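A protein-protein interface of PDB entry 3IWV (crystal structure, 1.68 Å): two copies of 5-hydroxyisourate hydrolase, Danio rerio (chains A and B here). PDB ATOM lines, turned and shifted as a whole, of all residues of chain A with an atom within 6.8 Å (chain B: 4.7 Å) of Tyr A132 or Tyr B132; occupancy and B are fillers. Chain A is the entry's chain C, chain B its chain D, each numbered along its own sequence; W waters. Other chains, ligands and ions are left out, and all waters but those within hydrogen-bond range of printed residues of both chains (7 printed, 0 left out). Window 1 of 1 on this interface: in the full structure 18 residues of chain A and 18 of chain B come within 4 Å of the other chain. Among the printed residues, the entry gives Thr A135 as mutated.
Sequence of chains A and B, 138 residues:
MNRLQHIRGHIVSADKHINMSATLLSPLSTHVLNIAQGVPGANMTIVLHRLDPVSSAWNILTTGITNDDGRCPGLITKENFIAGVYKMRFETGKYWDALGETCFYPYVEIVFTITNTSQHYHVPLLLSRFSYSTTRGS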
ATOM      1  N   ILE A  35      24.787 -10.262 -21.846  1.00  0.00           N
ATOM      2  CA  ILE A  35      26.112  -9.714 -22.070  1.00  0.00           C
ATOM      3  C   ILE A  35      27.215 -10.731 -22.014  1.00  0.00           C
ATOM      4  O   ILE A  35      28.385 -10.416 -22.322  1.00  0.00           O
ATOM      5  CB  ILE A  35      26.436  -8.493 -21.124  1.00  0.00           C
ATOM      6  CG1 ILE A  35      26.564  -8.981 -19.661  1.00  0.00           C
ATOM      7  CG2 ILE A  35      25.323  -7.477 -21.234  1.00  0.00           C
ATOM      8  CD1 ILE A  35      26.877  -7.842 -18.700  1.00  0.00           C
ATOM      9  N   THR A  92      15.051 -13.859 -13.732  1.00  0.00           N
ATOM     10  CA  THR A  92      16.387 -14.179 -14.247  1.00  0.00           C
ATOM     11  C   THR A  92      16.793 -15.624 -13.929  1.00  0.00           C
ATOM     12  O   THR A  92      17.446 -16.255 -14.751  1.00  0.00           O
ATOM     13  CB  THR A  92      17.443 -13.186 -13.704  1.00  0.00           C
ATOM     14  OG1 THR A  92      17.351 -13.196 -12.266  1.00  0.00           O
ATOM     15  CG2 THR A  92      17.131 -11.741 -14.249  1.00  0.00           C
ATOM     16  N   TYR A 105      21.529 -14.281  -9.218  1.00  0.00           N
ATOM     17  CA  TYR A 105      20.310 -13.516  -8.830  1.00  0.00           C
ATOM     18  C   TYR A 105      19.079 -14.258  -9.264  1.00  0.00           C
ATOM     19  O   TYR A 105      18.814 -14.338 -10.434  1.00  0.00           O
ATOM     20  CB  TYR A 105      20.325 -12.122  -9.488  1.00  0.00           C
ATOM     21  CG  TYR A 105      21.635 -11.407  -9.421  1.00  0.00           C
ATOM     22  CD1 TYR A 105      21.985 -10.628  -8.324  1.00  0.00           C
ATOM     23  CD2 TYR A 105      22.608 -11.590 -10.443  1.00  0.00           C
ATOM     24  CE1 TYR A 105      23.204  -9.993  -8.268  1.00  0.00           C
ATOM     25  CE2 TYR A 105      23.821 -10.985 -10.390  1.00  0.00           C
ATOM     26  CZ  TYR A 105      24.124 -10.207  -9.288  1.00  0.00           C
ATOM     27  OH  TYR A 105      25.320  -9.587  -9.242  1.00  0.00           O
ATOM     28  N   TYR A 107      15.965 -13.453  -9.126  1.00  0.00           N
ATOM     29  CA  TYR A 107      15.145 -12.585  -9.942  1.00  0.00           C
ATOM     30  C   TYR A 107      15.745 -11.188  -9.869  1.00  0.00           C
ATOM     31  O   TYR A 107      16.637 -10.939  -9.050  1.00  0.00           O
ATOM     32  CB  TYR A 107      13.668 -12.594  -9.504  1.00  0.00           C
ATOM     33  CG  TYR A 107      13.386 -12.069  -8.093  1.00  0.00           C
ATOM     34  CD1 TYR A 107      13.176 -12.935  -7.026  1.00  0.00           C
ATOM     35  CD2 TYR A 107      13.302 -10.725  -7.854  1.00  0.00           C
ATOM     36  CE1 TYR A 107      12.892 -12.485  -5.749  1.00  0.00           C
ATOM     37  CE2 TYR A 107      12.992 -10.252  -6.563  1.00  0.00           C
ATOM     38  CZ  TYR A 107      12.807 -11.097  -5.532  1.00  0.00           C
ATOM     39  OH  TYR A 107      12.545 -10.561  -4.269  1.00  0.00           O
ATOM     40  N   VAL A 108      15.243 -10.278 -10.706  1.00  0.00           N
ATOM     41  CA  VAL A 108      15.676  -8.859 -10.636  1.00  0.00           C
ATOM     42  C   VAL A 108      14.411  -7.981 -10.618  1.00  0.00           C
ATOM     43  O   VAL A 108      13.587  -8.068 -11.501  1.00  0.00           O
ATOM     44  CB  VAL A 108      16.543  -8.515 -11.844  1.00  0.00           C
ATOM     45  CG1 VAL A 108      16.675  -6.932 -12.057  1.00  0.00           C
ATOM     46  CG2 VAL A 108      17.922  -9.128 -11.643  1.00  0.00           C
ATOM     47  N   GLU A 109      14.278  -7.123  -9.608  1.00  0.00           N
ATOM     48  CA  GLU A 109      13.210  -6.188  -9.627  1.00  0.00           C
ATOM     49  C   GLU A 109      13.850  -4.837  -9.755  1.00  0.00           C
ATOM     50  O   GLU A 109      14.893  -4.579  -9.109  1.00  0.00           O
ATOM     51  CB  GLU A 109      12.375  -6.309  -8.360  1.00  0.00           C
ATOM     52  CG  GLU A 109      11.391  -7.516  -8.459  1.00  0.00           C
ATOM     53  CD  GLU A 109      10.563  -7.780  -7.199  1.00  0.00           C
ATOM     54  OE1 GLU A 109      10.742  -7.036  -6.199  1.00  0.00           O
ATOM     55  OE2 GLU A 109       9.710  -8.730  -7.222  1.00  0.00           O
ATOM     56  N   ILE A 110      13.286  -4.036 -10.669  1.00  0.00           N
ATOM     57  CA  ILE A 110      13.647  -2.632 -10.899  1.00  0.00           C
ATOM     58  C   ILE A 110      12.422  -1.814 -10.500  1.00  0.00           C
ATOM     59  O   ILE A 110      11.328  -1.951 -11.037  1.00  0.00           O
ATOM     60  CB  ILE A 110      13.995  -2.326 -12.363  1.00  0.00           C
ATOM     61  CG1 ILE A 110      15.196  -3.168 -12.794  1.00  0.00           C
ATOM     62  CG2 ILE A 110      14.478  -0.858 -12.493  1.00  0.00           C
ATOM     63  CD1 ILE A 110      15.640  -2.966 -14.228  1.00  0.00           C
ATOM     64  N   VAL A 111      12.626  -0.959  -9.531  1.00  0.00           N
ATOM     65  CA  VAL A 111      11.531  -0.118  -9.060  1.00  0.00           C
ATOM     66  C   VAL A 111      11.899   1.312  -9.401  1.00  0.00           C
ATOM     67  O   VAL A 111      12.999   1.792  -9.103  1.00  0.00           O
ATOM     68  CB  VAL A 111      11.376  -0.324  -7.568  1.00  0.00           C
ATOM     69  CG1 VAL A 111      10.352   0.663  -6.944  1.00  0.00           C
ATOM     70  CG2 VAL A 111      11.051  -1.815  -7.241  1.00  0.00           C
ATOM     71  N   LEU A 125      17.518  -4.396 -19.086  1.00  0.00           N
ATOM     72  CA  LEU A 125      18.267  -5.229 -18.122  1.00  0.00           C
ATOM     73  C   LEU A 125      19.412  -5.855 -18.908  1.00  0.00           C
ATOM     74  O   LEU A 125      19.152  -6.620 -19.820  1.00  0.00           O
ATOM     75  CB  LEU A 125      17.410  -6.292 -17.499  1.00  0.00           C
ATOM     76  CG  LEU A 125      18.129  -7.207 -16.469  1.00  0.00           C
ATOM     77  CD1 LEU A 125      18.643  -6.446 -15.219  1.00  0.00           C
ATOM     78  CD2 LEU A 125      17.129  -8.217 -15.999  1.00  0.00           C
ATOM     79  N   LEU A 126      20.636  -5.494 -18.576  1.00  0.00           N
ATOM     80  CA  LEU A 126      21.812  -6.024 -19.262  1.00  0.00           C
ATOM     81  C   LEU A 126      22.470  -6.994 -18.249  1.00  0.00           C
ATOM     82  O   LEU A 126      22.883  -6.586 -17.155  1.00  0.00           O
ATOM     83  CB  LEU A 126      22.704  -4.859 -19.620  1.00  0.00           C
ATOM     84  CG  LEU A 126      22.477  -4.121 -20.941  1.00  0.00           C
ATOM     85  CD1 LEU A 126      21.017  -3.629 -21.170  1.00  0.00           C
ATOM     86  CD2 LEU A 126      23.510  -2.967 -21.166  1.00  0.00           C
ATOM     87  N   LEU A 127      22.498  -8.288 -18.546  1.00  0.00           N
ATOM     88  CA  LEU A 127      22.783  -9.209 -17.451  1.00  0.00           C
ATOM     89  C   LEU A 127      23.696 -10.344 -17.883  1.00  0.00           C
ATOM     90  O   LEU A 127      23.725 -10.680 -19.068  1.00  0.00           O
ATOM     91  CB  LEU A 127      21.473  -9.787 -16.845  1.00  0.00           C
ATOM     92  CG  LEU A 127      20.749 -11.016 -17.419  1.00  0.00           C
ATOM     93  CD1 LEU A 127      19.576 -11.544 -16.589  1.00  0.00           C
ATOM     94  CD2 LEU A 127      20.240 -10.627 -18.804  1.00  0.00           C
ATOM     95  N   SER A 128      24.519 -10.813 -16.948  1.00  0.00           N
ATOM     96  CA  SER A 128      25.221 -12.099 -17.104  1.00  0.00           C
ATOM     97  C   SER A 128      24.784 -13.039 -16.002  1.00  0.00           C
ATOM     98  O   SER A 128      23.903 -12.716 -15.259  1.00  0.00           O
ATOM     99  CB  SER A 128      26.753 -11.889 -17.083  1.00  0.00           C
ATOM    100  OG  SER A 128      27.242 -11.679 -15.744  1.00  0.00           O
ATOM    101  N   PHE A 130      26.431 -13.424 -13.340  1.00  0.00           N
ATOM    102  CA  PHE A 130      26.956 -12.876 -12.125  1.00  0.00           C
ATOM    103  C   PHE A 130      27.071 -11.377 -12.081  1.00  0.00           C
ATOM    104  O   PHE A 130      27.891 -10.870 -11.322  1.00  0.00           O
ATOM    105  CB  PHE A 130      28.347 -13.494 -11.863  1.00  0.00           C
ATOM    106  CG  PHE A 130      28.278 -14.974 -11.643  1.00  0.00           C
ATOM    107  CD1 PHE A 130      27.921 -15.488 -10.407  1.00  0.00           C
ATOM    108  CD2 PHE A 130      28.573 -15.853 -12.700  1.00  0.00           C
ATOM    109  CE1 PHE A 130      27.824 -16.878 -10.207  1.00  0.00           C
ATOM    110  CE2 PHE A 130      28.484 -17.228 -12.538  1.00  0.00           C
ATOM    111  CZ  PHE A 130      28.127 -17.755 -11.294  1.00  0.00           C
ATOM    112  N   SER A 131      26.251 -10.696 -12.861  1.00  0.00           N
ATOM    113  CA  SER A 131      26.252  -9.211 -12.882  1.00  0.00           C
ATOM    114  C   SER A 131      24.981  -8.737 -13.559  1.00  0.00           C
ATOM    115  O   SER A 131      24.380  -9.501 -14.271  1.00  0.00           O
ATOM    116  CB  SER A 131      27.445  -8.632 -13.653  1.00  0.00           C
ATOM    117  OG  SER A 131      27.316  -8.641 -15.022  1.00  0.00           O
ATOM    118  N   TYR A 132      24.515  -7.515 -13.265  1.00  0.00           N
ATOM    119  CA  TYR A 132      23.552  -6.862 -14.170  1.00  0.00           C
ATOM    120  C   TYR A 132      23.565  -5.370 -13.984  1.00  0.00           C
ATOM    121  O   TYR A 132      24.037  -4.846 -12.940  1.00  0.00           O
ATOM    122  CB  TYR A 132      22.108  -7.317 -13.968  1.00  0.00           C
ATOM    123  CG  TYR A 132      21.443  -7.037 -12.610  1.00  0.00           C
ATOM    124  CD1 TYR A 132      21.565  -7.977 -11.509  1.00  0.00           C
ATOM    125  CD2 TYR A 132      20.732  -5.862 -12.357  1.00  0.00           C
ATOM    126  CE1 TYR A 132      20.949  -7.751 -10.228  1.00  0.00           C
ATOM    127  CE2 TYR A 132      20.059  -5.683 -11.129  1.00  0.00           C
ATOM    128  CZ  TYR A 132      20.222  -6.592 -10.053  1.00  0.00           C
ATOM    129  OH  TYR A 132      19.628  -6.452  -8.828  1.00  0.00           O
ATOM    130  N   SER A 133      22.950  -4.693 -14.950  1.00  0.00           N
ATOM    131  CA  SER A 133      22.900  -3.240 -14.917  1.00  0.00           C
ATOM    132  C   SER A 133      21.539  -2.778 -15.542  1.00  0.00           C
ATOM    133  O   SER A 133      20.880  -3.514 -16.287  1.00  0.00           O
ATOM    134  CB  SER A 133      24.140  -2.624 -15.596  1.00  0.00           C
ATOM    135  OG  SER A 133      24.096  -2.615 -16.998  1.00  0.00           O
ATOM    136  N   THR A 134      21.121  -1.590 -15.164  1.00  0.00           N
ATOM    137  CA  THR A 134      19.982  -0.985 -15.799  1.00  0.00           C
ATOM    138  C   THR A 134      20.270   0.527 -15.872  1.00  0.00           C
ATOM    139  O   THR A 134      21.123   1.040 -15.174  1.00  0.00           O
ATOM    140  CB  THR A 134      18.676  -1.228 -15.031  1.00  0.00           C
ATOM    141  OG1 THR A 134      17.578  -0.815 -15.891  1.00  0.00           O
ATOM    142  CG2 THR A 134      18.625  -0.436 -13.624  1.00  0.00           C
ATOM    143  N   THR A 135      19.596   1.197 -16.774  1.00  0.00           N
ATOM    144  CA  THR A 135      19.688   2.671 -16.957  1.00  0.00           C
ATOM    145  C   THR A 135      18.271   3.157 -17.283  1.00  0.00           C
ATOM    146  O   THR A 135      17.396   2.368 -17.713  1.00  0.00           O
ATOM    147  CB  THR A 135      20.575   3.026 -18.156  1.00  0.00           C
ATOM    148  OG1 THR A 135      20.165   2.240 -19.304  1.00  0.00           O
ATOM    149  CG2 THR A 135      22.087   2.721 -17.874  1.00  0.00           C
ATOM    150  N   ARG A 136      18.001   4.436 -16.971  1.00  0.00           N
ATOM    151  CA  ARG A 136      16.843   5.087 -17.538  1.00  0.00           C
ATOM    152  C   ARG A 136      17.220   5.683 -18.913  1.00  0.00           C
ATOM    153  O   ARG A 136      18.173   6.430 -19.013  1.00  0.00           O
ATOM    154  CB  ARG A 136      16.310   6.212 -16.618  1.00  0.00           C
ATOM    155  CG  ARG A 136      14.941   6.673 -17.065  1.00  0.00           C
ATOM    156  CD  ARG A 136      15.006   7.496 -18.343  1.00  0.00           C
ATOM    157  NE  ARG A 136      14.713   8.877 -18.106  1.00  0.00           N
ATOM    158  CZ  ARG A 136      13.780   9.571 -18.747  1.00  0.00           C
ATOM    159  NH1 ARG A 136      13.048   9.024 -19.712  1.00  0.00           N
ATOM    160  NH2 ARG A 136      13.604  10.840 -18.418  1.00  0.00           N
ATOM    161  N   TYR B 105      15.129   5.683  -9.029  1.00  0.00           N
ATOM    162  CA  TYR B 105      14.790   4.514  -8.262  1.00  0.00           C
ATOM    163  C   TYR B 105      14.589   4.835  -6.786  1.00  0.00           C
ATOM    164  O   TYR B 105      15.552   5.229  -6.077  1.00  0.00           O
ATOM    165  CB  TYR B 105      15.903   3.475  -8.363  1.00  0.00           C
ATOM    166  CG  TYR B 105      16.434   3.332  -9.747  1.00  0.00           C
ATOM    167  CD1 TYR B 105      15.779   2.548 -10.705  1.00  0.00           C
ATOM    168  CD2 TYR B 105      17.661   3.913 -10.102  1.00  0.00           C
ATOM    169  CE1 TYR B 105      16.282   2.435 -11.976  1.00  0.00           C
ATOM    170  CE2 TYR B 105      18.150   3.837 -11.386  1.00  0.00           C
ATOM    171  CZ  TYR B 105      17.484   3.041 -12.308  1.00  0.00           C
ATOM    172  OH  TYR B 105      17.976   2.917 -13.559  1.00  0.00           O
ATOM    173  N   VAL B 108      16.753   0.342  -4.306  1.00  0.00           N
ATOM    174  CA  VAL B 108      17.258  -0.740  -5.179  1.00  0.00           C
ATOM    175  C   VAL B 108      17.352  -2.020  -4.287  1.00  0.00           C
ATOM    176  O   VAL B 108      17.887  -1.911  -3.188  1.00  0.00           O
ATOM    177  CB  VAL B 108      18.653  -0.341  -5.704  1.00  0.00           C
ATOM    178  CG1 VAL B 108      19.259  -1.533  -6.422  1.00  0.00           C
ATOM    179  CG2 VAL B 108      18.543   0.827  -6.759  1.00  0.00           C
ATOM    180  N   GLU B 109      16.906  -3.189  -4.763  1.00  0.00           N
ATOM    181  CA  GLU B 109      17.025  -4.421  -4.008  1.00  0.00           C
ATOM    182  C   GLU B 109      17.811  -5.360  -4.871  1.00  0.00           C
ATOM    183  O   GLU B 109      17.485  -5.485  -6.048  1.00  0.00           O
ATOM    184  CB  GLU B 109      15.637  -5.026  -3.722  1.00  0.00           C
ATOM    185  CG  GLU B 109      14.947  -4.282  -2.563  1.00  0.00           C
ATOM    186  CD  GLU B 109      13.553  -4.853  -2.180  1.00  0.00           C
ATOM    187  OE1 GLU B 109      12.847  -5.481  -3.004  1.00  0.00           O
ATOM    188  OE2 GLU B 109      13.150  -4.652  -1.026  1.00  0.00           O
ATOM    189  N   ILE B 110      18.872  -5.956  -4.312  1.00  0.00           N
ATOM    190  CA  ILE B 110      19.632  -6.955  -5.038  1.00  0.00           C
ATOM    191  C   ILE B 110      19.357  -8.278  -4.333  1.00  0.00           C
ATOM    192  O   ILE B 110      19.661  -8.391  -3.138  1.00  0.00           O
ATOM    193  CB  ILE B 110      21.156  -6.638  -4.988  1.00  0.00           C
ATOM    194  CG1 ILE B 110      21.478  -5.192  -5.451  1.00  0.00           C
ATOM    195  CG2 ILE B 110      21.912  -7.598  -5.847  1.00  0.00           C
ATOM    196  CD1 ILE B 110      20.784  -4.812  -6.708  1.00  0.00           C
ATOM    197  N   LEU B 125      27.040  -1.835  -5.024  1.00  0.00           N
ATOM    198  CA  LEU B 125      26.105  -1.069  -5.806  1.00  0.00           C
ATOM    199  C   LEU B 125      26.866   0.116  -6.411  1.00  0.00           C
ATOM    200  O   LEU B 125      27.433   0.937  -5.690  1.00  0.00           O
ATOM    201  CB  LEU B 125      24.892  -0.555  -5.019  1.00  0.00           C
ATOM    202  CG  LEU B 125      23.859   0.186  -5.908  1.00  0.00           C
ATOM    203  CD1 LEU B 125      23.088  -0.714  -6.843  1.00  0.00           C
ATOM    204  CD2 LEU B 125      22.812   0.861  -4.936  1.00  0.00           C
ATOM    205  N   LEU B 126      26.829   0.215  -7.733  1.00  0.00           N
ATOM    206  CA  LEU B 126      27.490   1.298  -8.455  1.00  0.00           C
ATOM    207  C   LEU B 126      26.352   2.115  -9.070  1.00  0.00           C
ATOM    208  O   LEU B 126      25.586   1.640  -9.940  1.00  0.00           O
ATOM    209  CB  LEU B 126      28.471   0.729  -9.509  1.00  0.00           C
ATOM    210  CG  LEU B 126      29.914   0.292  -9.155  1.00  0.00           C
ATOM    211  CD1 LEU B 126      30.021  -0.745  -8.019  1.00  0.00           C
ATOM    212  CD2 LEU B 126      30.651  -0.241 -10.381  1.00  0.00           C
ATOM    213  N   LEU B 127      26.139   3.346  -8.596  1.00  0.00           N
ATOM    214  CA  LEU B 127      24.901   3.966  -9.024  1.00  0.00           C
ATOM    215  C   LEU B 127      25.100   5.452  -9.405  1.00  0.00           C
ATOM    216  O   LEU B 127      26.050   6.106  -8.924  1.00  0.00           O
ATOM    217  CB  LEU B 127      23.807   3.809  -7.940  1.00  0.00           C
ATOM    218  CG  LEU B 127      23.712   4.900  -6.885  1.00  0.00           C
ATOM    219  CD1 LEU B 127      22.444   4.876  -6.058  1.00  0.00           C
ATOM    220  CD2 LEU B 127      24.926   4.833  -5.963  1.00  0.00           C
ATOM    221  N   SER B 131      20.966   5.266 -13.143  1.00  0.00           N
ATOM    222  CA  SER B 131      21.514   3.937 -13.575  1.00  0.00           C
ATOM    223  C   SER B 131      22.001   3.149 -12.355  1.00  0.00           C
ATOM    224  O   SER B 131      22.305   3.710 -11.346  1.00  0.00           O
ATOM    225  CB  SER B 131      22.671   4.063 -14.571  1.00  0.00           C
ATOM    226  OG  SER B 131      23.861   4.588 -13.996  1.00  0.00           O
ATOM    227  N   TYR B 132      22.140   1.827 -12.452  1.00  0.00           N
ATOM    228  CA  TYR B 132      22.937   1.225 -11.388  1.00  0.00           C
ATOM    229  C   TYR B 132      23.392  -0.086 -11.921  1.00  0.00           C
ATOM    230  O   TYR B 132      22.765  -0.578 -12.851  1.00  0.00           O
ATOM    231  CB  TYR B 132      22.180   1.082 -10.058  1.00  0.00           C
ATOM    232  CG  TYR B 132      20.968   0.202 -10.037  1.00  0.00           C
ATOM    233  CD1 TYR B 132      19.693   0.733 -10.261  1.00  0.00           C
ATOM    234  CD2 TYR B 132      21.074  -1.197  -9.784  1.00  0.00           C
ATOM    235  CE1 TYR B 132      18.540  -0.083 -10.233  1.00  0.00           C
ATOM    236  CE2 TYR B 132      19.925  -1.990  -9.728  1.00  0.00           C
ATOM    237  CZ  TYR B 132      18.657  -1.405  -9.944  1.00  0.00           C
ATOM    238  OH  TYR B 132      17.518  -2.113  -9.894  1.00  0.00           O
ATOM    239  N   SER B 133      24.472  -0.600 -11.317  1.00  0.00           N
ATOM    240  CA  SER B 133      24.968  -1.977 -11.696  1.00  0.00           C
ATOM    241  C   SER B 133      25.419  -2.730 -10.441  1.00  0.00           C
ATOM    242  O   SER B 133      25.770  -2.116  -9.417  1.00  0.00           O
ATOM    243  CB  SER B 133      26.116  -1.924 -12.736  1.00  0.00           C
ATOM    244  OG  SER B 133      27.302  -1.267 -12.308  1.00  0.00           O
ATOM    245  N   THR B 134      25.533  -4.047 -10.576  1.00  0.00           N
ATOM    246  CA  THR B 134      26.102  -4.854  -9.475  1.00  0.00           C
ATOM    247  C   THR B 134      26.793  -6.047 -10.092  1.00  0.00           C
ATOM    248  O   THR B 134      26.473  -6.396 -11.204  1.00  0.00           O
ATOM    249  CB  THR B 134      25.011  -5.303  -8.493  1.00  0.00           C
ATOM    250  OG1 THR B 134      25.614  -5.895  -7.295  1.00  0.00           O
ATOM    251  CG2 THR B 134      23.930  -6.191  -9.144  1.00  0.00           C
HETATM  252  O   HOH W   1      17.509  -4.382  -8.836  1.00  0.00           O
HETATM  253  O   HOH W   2      14.863  -3.013  -6.905  1.00  0.00           O
HETATM  254  O   HOH W   3      15.734  -7.278  -7.134  1.00  0.00           O
HETATM  255  O   HOH W   4      11.694  -4.592  -5.190  1.00  0.00           O
HETATM  256  O   HOH W   5      16.329   1.426 -15.094  1.00  0.00           O
HETATM  257  O   HOH W   6      25.850  -8.504  -6.954  1.00  0.00           O
HETATM  258  O   HOH W   7      15.257  -0.581  -8.229  1.00  0.00           O
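The backbone carbonyl oxygen (O) of Tyr A132 is in hydrogen-bond range of the backbone NH (N) of Thr B134 (2.9 Å).
The backbone carbonyl oxygen (O) of Thr A134 sits at hydrogen-bond distance from the backbone NH (N) of Tyr B132.
O of Tyr A105 sits at hydrogen-bond distance from OG1 of Thr A92.
The backbone carbonyl oxygen (O) of Leu A126 lies within hydrogen-bond range of the backbone NH (N) of Ser A133 (2.9 Å).
The side-chain hydroxyl of Ser A131 sits at hydrogen-bond distance from the side-chain hydroxyl of Ser A128, at 3.1 Å.
O of Leu B126 sits at hydrogen-bond distance from N of Ser B133, at 2.9 Å.
Among the printed residues, pairs that only touch across the chains: Tyr A132 with Ile B110, Tyr A132 with Ser B133, Ser A131 with Thr B134, Val A111 with Tyr B105, Thr A134 with Ser B131, Ser A133 with Tyr B132, Thr A134 with Tyr B105, Ser A133 with Ser B133, Thr A135 with Ser B131, Tyr A132 with Glu B109, Tyr A105 with Ile B110, Tyr A105 with Thr B134, Glu A109 with Tyr B132, Arg A136 with Tyr B105, Thr A135 with Tyr B105, Ile A110 with Tyr B105, Ile A110 with Tyr B132 and Tyr A132 with Tyr B132.
Printed residues of chain B within 4 Å of Ser A131: Thr B134 (3.3 Å).
Of chain B, only Glu B109 (3.6 Å), Ile B110 (2.9 Å), Tyr B132 (3.95 Å), Ser B133 (3.3 Å) and Thr B134 (2.9 Å) come within 4 Å of Tyr A132.
Of the printed residues of chain B, Thr A135 touches Tyr B105 (3.7 Å) and Ser B131 (3.6 Å).
Of the printed residues of chain A, Ile B110 touches Tyr A105 and Tyr A132.
Leu B126 touches none of the printed residues of chain A.
Tyr B132 touches five residues of chain A.
The nearest printed residue of chain A that does not touch Tyr B132 is Val A111 (5.0 Å).
The nearest printed residue of chain B that does not touch Tyr A105 is Ser B133 (7.0 Å).
Of the 11 printed residues of chain B, 7 touch a printed residue of chain A.
Hydrophobic or aromatic side chains of chain B that line the printed part of chain A: Tyr B105, Ile B110 and Tyr B132.
Printed residues of chain A that touch a printed residue of chain B: Tyr A105, Glu A109, Ile A110, Val A111, Ser A131, Tyr A132, Ser A133, Thr A134, Thr A135 and Arg A136.
Hydrophobic or aromatic side chains of chain A that line the printed part of chain B: Tyr A105, Ile A110 and Tyr A132.
Among the printed residues, 20 pairs touch across the chains.
Among the printed residues, no Asp or Glu carboxylate lies within 4 Å of a Lys or Arg side-chain nitrogen of the other chain.
Tyr A105 touches Ile B110, and with the chains exchanged Ile A110 touches Tyr B105.
Tyr A105 touches Thr B134, and with the chains exchanged Thr A134 touches Tyr B105.
Ile A110 touches Tyr B132, and with the chains exchanged Tyr A132 touches Ile B110.
Tyr A132 touches Ser B133, and with the chains exchanged Ser A133 touches Tyr B132.
11 positions are printed for both chains.
Of the 20 pairs that touch across the chains among the printed residues, 16 have their exchanged pair printed and touching as well.
Water W1 lies within hydrogen-bond range of the side-chain hydroxyl of Tyr B132 (2.5 Å), the backbone carbonyl oxygen of Glu A109 (2.6 Å), the side-chain hydroxyl of Tyr A132 (3.0 Å) and the backbone carbonyl oxygen of Glu B109 (3.0 Å).
Water W4 bridges the side-chain carboxylate of Glu B109 (2.6 Å) and the side-chain carboxylate of Glu A109 (2.8 Å).
Water W5 lies within hydrogen-bond range of OG1 of Thr A134, OH of Tyr B105 and O of Thr A135.
Water W2 lies within hydrogen-bond range of O of Glu A109 (2.7 Å) and N of Glu B109 (3.0 Å).
Water W3 bridges the backbone carbonyl oxygen (O) of Glu B109 (2.7 Å) and the backbone NH (N) of Glu A109 (2.9 Å).
Water W7 lies within hydrogen-bond range of N of Val A111 (3.0 Å) and OH of Tyr B132 (3.2 Å).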
